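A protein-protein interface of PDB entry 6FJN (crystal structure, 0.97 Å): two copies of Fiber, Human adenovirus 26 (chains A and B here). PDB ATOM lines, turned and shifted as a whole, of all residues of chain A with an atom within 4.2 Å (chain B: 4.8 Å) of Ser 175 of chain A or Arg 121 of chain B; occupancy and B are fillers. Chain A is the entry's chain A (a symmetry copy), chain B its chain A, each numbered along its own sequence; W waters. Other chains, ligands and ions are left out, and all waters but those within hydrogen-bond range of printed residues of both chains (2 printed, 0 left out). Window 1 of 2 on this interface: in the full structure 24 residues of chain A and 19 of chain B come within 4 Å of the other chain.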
ATOM      1  N   PRO A   8       4.431  15.213  -4.125  1.00  0.00           N
ATOM      2  CA  PRO A   8       4.858  13.927  -3.569  1.00  0.00           C
ATOM      3  C   PRO A   8       4.219  12.721  -4.249  1.00  0.00           C
ATOM      4  O   PRO A   8       4.219  11.639  -3.671  1.00  0.00           O
ATOM      5  CB  PRO A   8       4.303  14.014  -2.137  1.00  0.00           C
ATOM      6  CG  PRO A   8       3.066  14.798  -2.264  1.00  0.00           C
ATOM      7  CD  PRO A   8       3.410  15.859  -3.283  1.00  0.00           C
ATOM      8  N   ASP A   9       3.633  12.871  -5.433  1.00  0.00           N
ATOM      9  CA  ASP A   9       3.024  11.714  -6.110  1.00  0.00           C
ATOM     10  C   ASP A   9       4.120  10.897  -6.780  1.00  0.00           C
ATOM     11  O   ASP A   9       5.287  11.175  -6.567  1.00  0.00           O
ATOM     12  CB  ASP A   9       1.933  12.177  -7.093  1.00  0.00           C
ATOM     13  CG  ASP A   9       2.459  12.987  -8.297  1.00  0.00           C
ATOM     14  OD1 ASP A   9       3.649  12.920  -8.620  1.00  0.00           O
ATOM     15  OD2 ASP A   9       1.630  13.632  -8.993  1.00  0.00           O
ATOM     16  N   THR A  10       3.734   9.882  -7.574  1.00  0.00           N
ATOM     17  CA  THR A  10       4.712   9.080  -8.291  1.00  0.00           C
ATOM     18  C   THR A  10       4.632   9.256  -9.813  1.00  0.00           C
ATOM     19  O   THR A  10       5.135   8.397 -10.553  1.00  0.00           O
ATOM     20  CB  THR A  10       4.599   7.589  -7.902  1.00  0.00           C
ATOM     21  OG1 THR A  10       3.259   7.121  -8.083  1.00  0.00           O
ATOM     22  CG2 THR A  10       5.055   7.408  -6.457  1.00  0.00           C
ATOM     23  N   THR A  25      11.577  12.891  -6.584  1.00  0.00           N
ATOM     24  CA  THR A  25      10.839  13.519  -5.508  1.00  0.00           C
ATOM     25  C   THR A  25      11.756  14.531  -4.872  1.00  0.00           C
ATOM     26  O   THR A  25      12.769  14.146  -4.307  1.00  0.00           O
ATOM     27  CB  THR A  25      10.323  12.516  -4.482  1.00  0.00           C
ATOM     28  OG1 THR A  25       9.576  11.502  -5.143  1.00  0.00           O
ATOM     29  CG2 THR A  25       9.432  13.183  -3.441  1.00  0.00           C
ATOM     30  N   VAL A  39      15.319  14.708  -1.051  1.00  0.00           N
ATOM     31  CA  VAL A  39      15.318  14.172  -2.423  1.00  0.00           C
ATOM     32  C   VAL A  39      15.300  12.656  -2.418  1.00  0.00           C
ATOM     33  O   VAL A  39      15.951  11.987  -1.567  1.00  0.00           O
ATOM     34  CB  VAL A  39      16.538  14.710  -3.214  1.00  0.00           C
ATOM     35  CG1 VAL A  39      17.864  14.259  -2.649  1.00  0.00           C
ATOM     36  CG2 VAL A  39      16.437  14.401  -4.720  1.00  0.00           C
ATOM     37  N   SER A  40      14.755  12.111  -3.494  1.00  0.00           N
ATOM     38  CA  SER A  40      14.861  10.712  -3.804  1.00  0.00           C
ATOM     39  C   SER A  40      14.503  10.550  -5.271  1.00  0.00           C
ATOM     40  O   SER A  40      13.967  11.491  -5.915  1.00  0.00           O
ATOM     41  CB  SER A  40      13.874   9.920  -2.947  1.00  0.00           C
ATOM     42  OG  SER A  40      12.512  10.268  -3.223  1.00  0.00           O
ATOM     43  N   VAL A 173      15.749   4.704  -4.507  1.00  0.00           N
ATOM     44  CA  VAL A 173      16.628   4.974  -3.365  1.00  0.00           C
ATOM     45  C   VAL A 173      15.895   5.591  -2.216  1.00  0.00           C
ATOM     46  O   VAL A 173      14.835   6.238  -2.375  1.00  0.00           O
ATOM     47  CB  VAL A 173      17.841   5.847  -3.771  1.00  0.00           C
ATOM     48  CG1 VAL A 173      18.800   5.093  -4.647  1.00  0.00           C
ATOM     49  CG2 VAL A 173      17.400   7.174  -4.397  1.00  0.00           C
ATOM     50  N   THR A 174      16.436   5.395  -1.026  1.00  0.00           N
ATOM     51  CA  THR A 174      15.962   6.061   0.171  1.00  0.00           C
ATOM     52  C   THR A 174      16.057   7.574   0.039  1.00  0.00           C
ATOM     53  O   THR A 174      16.766   8.118  -0.807  1.00  0.00           O
ATOM     54  CB  THR A 174      16.758   5.559   1.392  1.00  0.00           C
ATOM     55  OG1 THR A 174      18.159   5.707   1.152  1.00  0.00           O
ATOM     56  CG2 THR A 174      16.446   4.117   1.677  1.00  0.00           C
ATOM     57  N   SER A 175      15.302   8.260   0.910  1.00  0.00           N
ATOM     58  CA  SER A 175      15.270   9.718   0.922  1.00  0.00           C
ATOM     59  C   SER A 175      16.506  10.298   1.575  1.00  0.00           C
ATOM     60  O   SER A 175      17.026   9.737   2.561  1.00  0.00           O
ATOM     61  CB  SER A 175      14.031  10.203   1.652  1.00  0.00           C
ATOM     62  OG  SER A 175      12.836   9.935   0.933  1.00  0.00           O
ATOM     63  N   PHE A 176      16.922  11.463   1.096  1.00  0.00           N
ATOM     64  CA  PHE A 176      18.111  12.132   1.609  1.00  0.00           C
ATOM     65  C   PHE A 176      17.819  13.585   1.932  1.00  0.00           C
ATOM     66  O   PHE A 176      17.297  14.335   1.073  1.00  0.00           O
ATOM     67  CB  PHE A 176      19.229  12.055   0.566  1.00  0.00           C
ATOM     68  CG  PHE A 176      20.553  12.573   1.088  1.00  0.00           C
ATOM     69  CD1 PHE A 176      21.258  11.874   2.030  1.00  0.00           C
ATOM     70  CD2 PHE A 176      21.080  13.783   0.625  1.00  0.00           C
ATOM     71  CE1 PHE A 176      22.443  12.330   2.500  1.00  0.00           C
ATOM     72  CE2 PHE A 176      22.278  14.274   1.099  1.00  0.00           C
ATOM     73  CZ  PHE A 176      22.951  13.551   2.060  1.00  0.00           C
ATOM     74  N   THR B 106       0.720  10.813   0.925  1.00  0.00           N
ATOM     75  CA  THR B 106       0.989  10.673  -0.520  1.00  0.00           C
ATOM     76  C   THR B 106       2.444  10.347  -0.780  1.00  0.00           C
ATOM     77  O   THR B 106       2.807   9.428  -1.537  1.00  0.00           O
ATOM     78  CB  THR B 106       0.601  11.921  -1.296  1.00  0.00           C
ATOM     79  OG1 THR B 106      -0.772  12.185  -1.023  1.00  0.00           O
ATOM     80  CG2 THR B 106       0.800  11.741  -2.795  1.00  0.00           C
ATOM     81  N   ALA B 107       3.358  11.054  -0.101  1.00  0.00           N
ATOM     82  CA  ALA B 107       4.795  10.750  -0.202  1.00  0.00           C
ATOM     83  C   ALA B 107       5.073   9.368   0.350  1.00  0.00           C
ATOM     84  O   ALA B 107       5.924   8.593  -0.157  1.00  0.00           O
ATOM     85  CB  ALA B 107       5.592  11.763   0.590  1.00  0.00           C
ATOM     86  N   TYR B 108       4.401   9.066   1.477  1.00  0.00           N
ATOM     87  CA  TYR B 108       4.714   7.856   2.258  1.00  0.00           C
ATOM     88  C   TYR B 108       3.439   7.078   2.500  1.00  0.00           C
ATOM     89  O   TYR B 108       2.838   7.136   3.587  1.00  0.00           O
ATOM     90  CB  TYR B 108       5.436   8.189   3.571  1.00  0.00           C
ATOM     91  CG  TYR B 108       6.448   9.291   3.465  1.00  0.00           C
ATOM     92  CD1 TYR B 108       7.557   9.188   2.676  1.00  0.00           C
ATOM     93  CD2 TYR B 108       6.297  10.476   4.190  1.00  0.00           C
ATOM     94  CE1 TYR B 108       8.506  10.196   2.608  1.00  0.00           C
ATOM     95  CE2 TYR B 108       7.236  11.493   4.133  1.00  0.00           C
ATOM     96  CZ  TYR B 108       8.338  11.358   3.349  1.00  0.00           C
ATOM     97  OH  TYR B 108       9.246  12.395   3.290  1.00  0.00           O
ATOM     98  N   TYR B 119       7.698   2.100  -2.008  1.00  0.00           N
ATOM     99  CA  TYR B 119       8.659   3.011  -2.481  1.00  0.00           C
ATOM    100  C   TYR B 119       9.801   3.198  -1.506  1.00  0.00           C
ATOM    101  O   TYR B 119       9.555   3.405  -0.324  1.00  0.00           O
ATOM    102  CB  TYR B 119       7.877   4.306  -2.657  1.00  0.00           C
ATOM    103  CG  TYR B 119       6.843   4.154  -3.745  1.00  0.00           C
ATOM    104  CD1 TYR B 119       7.259   3.881  -5.020  1.00  0.00           C
ATOM    105  CD2 TYR B 119       5.428   4.174  -3.519  1.00  0.00           C
ATOM    106  CE1 TYR B 119       6.379   3.703  -6.077  1.00  0.00           C
ATOM    107  CE2 TYR B 119       4.531   3.992  -4.582  1.00  0.00           C
ATOM    108  CZ  TYR B 119       5.039   3.763  -5.848  1.00  0.00           C
ATOM    109  OH  TYR B 119       4.196   3.568  -6.921  1.00  0.00           O
ATOM    110  N   SER B 120      11.045   3.183  -1.996  1.00  0.00           N
ATOM    111  CA  SER B 120      12.188   3.343  -1.100  1.00  0.00           C
ATOM    112  C   SER B 120      12.218   4.710  -0.417  1.00  0.00           C
ATOM    113  O   SER B 120      12.844   4.827   0.610  1.00  0.00           O
ATOM    114  CB  SER B 120      13.490   3.073  -1.844  1.00  0.00           C
ATOM    115  OG  SER B 120      13.497   1.782  -2.411  1.00  0.00           O
ATOM    116  N   ARG B 121      11.549   5.705  -1.013  1.00  0.00           N
ATOM    117  CA  ARG B 121      11.556   7.027  -0.399  1.00  0.00           C
ATOM    118  C   ARG B 121      10.858   7.055   0.961  1.00  0.00           C
ATOM    119  O   ARG B 121      11.050   8.001   1.731  1.00  0.00           O
ATOM    120  CB  ARG B 121      10.923   8.068  -1.316  1.00  0.00           C
ATOM    121  CG  ARG B 121       9.408   7.952  -1.474  1.00  0.00           C
ATOM    122  CD  ARG B 121       8.877   8.952  -2.476  1.00  0.00           C
ATOM    123  NE  ARG B 121       7.429   8.867  -2.527  1.00  0.00           N
ATOM    124  CZ  ARG B 121       6.655   9.396  -3.429  1.00  0.00           C
ATOM    125  NH1 ARG B 121       7.099  10.188  -4.410  1.00  0.00           N
ATOM    126  NH2 ARG B 121       5.355   9.126  -3.358  1.00  0.00           N
ATOM    127  N   THR B 122      10.095   6.023   1.298  1.00  0.00           N
ATOM    128  CA  THR B 122       9.486   5.882   2.629  1.00  0.00           C
ATOM    129  C   THR B 122      10.483   5.621   3.731  1.00  0.00           C
ATOM    130  O   THR B 122      10.059   5.632   4.896  1.00  0.00           O
ATOM    131  CB  THR B 122       8.409   4.792   2.630  1.00  0.00           C
ATOM    132  OG1 THR B 122       8.998   3.519   2.412  1.00  0.00           O
ATOM    133  CG2 THR B 122       7.289   5.057   1.633  1.00  0.00           C
ATOM    134  N   LYS B 123      11.747   5.406   3.394  1.00  0.00           N
ATOM    135  CA  LYS B 123      12.777   5.162   4.385  1.00  0.00           C
ATOM    136  C   LYS B 123      13.932   6.133   4.189  1.00  0.00           C
ATOM    137  O   LYS B 123      14.220   6.598   3.085  1.00  0.00           O
ATOM    138  CB  LYS B 123      13.283   3.725   4.322  1.00  0.00           C
ATOM    139  CG  LYS B 123      12.256   2.747   4.834  1.00  0.00           C
ATOM    140  CD  LYS B 123      12.688   1.315   4.727  1.00  0.00           C
ATOM    141  CE  LYS B 123      11.709   0.340   5.345  1.00  0.00           C
ATOM    142  NZ  LYS B 123      12.192  -1.071   5.274  1.00  0.00           N
ATOM    143  N   ILE B 124      14.624   6.358   5.307  1.00  0.00           N
ATOM    144  CA  ILE B 124      15.944   6.976   5.383  1.00  0.00           C
ATOM    145  C   ILE B 124      16.870   5.938   5.974  1.00  0.00           C
ATOM    146  O   ILE B 124      16.518   5.353   7.018  1.00  0.00           O
ATOM    147  CB  ILE B 124      15.954   8.229   6.272  1.00  0.00           C
ATOM    148  CG1 ILE B 124      14.982   9.263   5.762  1.00  0.00           C
ATOM    149  CG2 ILE B 124      17.357   8.758   6.435  1.00  0.00           C
ATOM    150  CD1 ILE B 124      14.628  10.237   6.870  1.00  0.00           C
HETATM  151  O   HOH W   1      11.626   9.470   4.003  1.00  0.00           O
HETATM  152  O   HOH W   2      10.944  11.979   1.244  1.00  0.00           O
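Among the printed residues, pairs that only touch across the chains: Pro 8 of chain A with Ala 107 of chain B (3.6 Å), Asp 9 of chain A with Thr 106 of chain B (3.99 Å), Thr 10 of chain A with Tyr 119 of chain B (3.7 Å), Thr 10 of chain A with Arg 121 of chain B (3.6 Å), Ser 40 of chain A with Arg 121 of chain B (3.3 Å), Val 173 of chain A with Ser 120 of chain B (3.5 Å), Val 173 of chain A with Arg 121 of chain B (3.6 Å), Thr 174 of chain A with Ser 120 of chain B (3.4 Å), Thr 174 of chain A with Lys 123 of chain B (3.2 Å) and Ser 175 of chain A with Ile 124 of chain B (3.8 Å).
Printed residues of chain B within 4 Å of Ser 175 of chain A: Arg 121, Lys 123 and Ile 124. Of the printed residues of chain A, Arg 121 of chain B touches Pro 8, Asp 9, Thr 10, Thr 25, Ser 40, Val 173 and Ser 175. Of the printed residues of chain B, Val 173 of chain A touches Ser 120 (3.5 Å) and Arg 121 (3.6 Å). Printed residues of chain B within 4 Å of Thr 174 of chain A: Ser 120 (3.4 Å) and Lys 123 (3.2 Å). Of the printed residues of chain A, Ser 120 of chain B touches Val 173 (3.5 Å) and Thr 174 (3.4 Å). Of the printed residues of chain B, Pro 8 of chain A touches Thr 106 (3.4 Å), Ala 107 (3.6 Å) and Arg 121 (2.8 Å). Of the printed residues of chain B, Ser 40 of chain A touches Arg 121. The nearest printed residue of chain B that does not touch Ser 40 of chain A is Ser 120 of chain B (6.0 Å).
The side-chain hydroxyl of Thr 122 of chain B is in hydrogen-bond range of the backbone carbonyl oxygen of Tyr 119 of chain B (2.8 Å). NE of Arg 121 of chain B sits at hydrogen-bond distance from O of Ala 107 of chain B (2.8 Å). The backbone carbonyl oxygen (O) of Thr 106 of chain B lies within hydrogen-bond range of the guanidinium group (NH2) of Arg 121 of chain B, at 3.1 Å. N of Thr 25 of chain A is in hydrogen-bond range of O of Ser 40 of chain A, 2.8 Å away.
Hydrophobic or aromatic side chains of chain A within 4 Å of the printed part of chain B: Pro 8. Along chain A the printed residues that touch a printed residue of chain B span positions 8 to 175.
Water W2 bridges OH of Tyr 108 of chain B (2.7 Å) and OG of Ser 175 of chain A (2.8 Å). Water W1 bridges the backbone carbonyl oxygen of Arg 121 of chain B (2.8 Å) and the side-chain hydroxyl of Ser 175 of chain A (3.3 Å).
No position is printed for both chains. Of the 16 pairs that touch across the chains among the printed residues, none has its exchanged pair printed and touching as well.
The backbone carbonyl oxygen of Lys 123 of chain B lies within hydrogen-bond range of the backbone NH of Ser 175 of chain A, at 2.9 Å. O of Asp 9 of chain A is in hydrogen-bond range of NH1 of Arg 121 of chain B, 3.0 Å away. The backbone carbonyl oxygen of Pro 8 of chain A lies within hydrogen-bond range of the guanidinium group of Arg 121 of chain B, at 2.8 Å. O of Arg 121 of chain B lies within hydrogen-bond range of OG of Ser 175 of chain A, at 2.8 Å. O of Thr 106 of chain B sits close to O of Pro 8 of chain A. The side-chain hydroxyl (OG1) of Thr 25 of chain A lies within hydrogen-bond range of the guanidinium group (NH1) of Arg 121 of chain B (2.9 Å).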
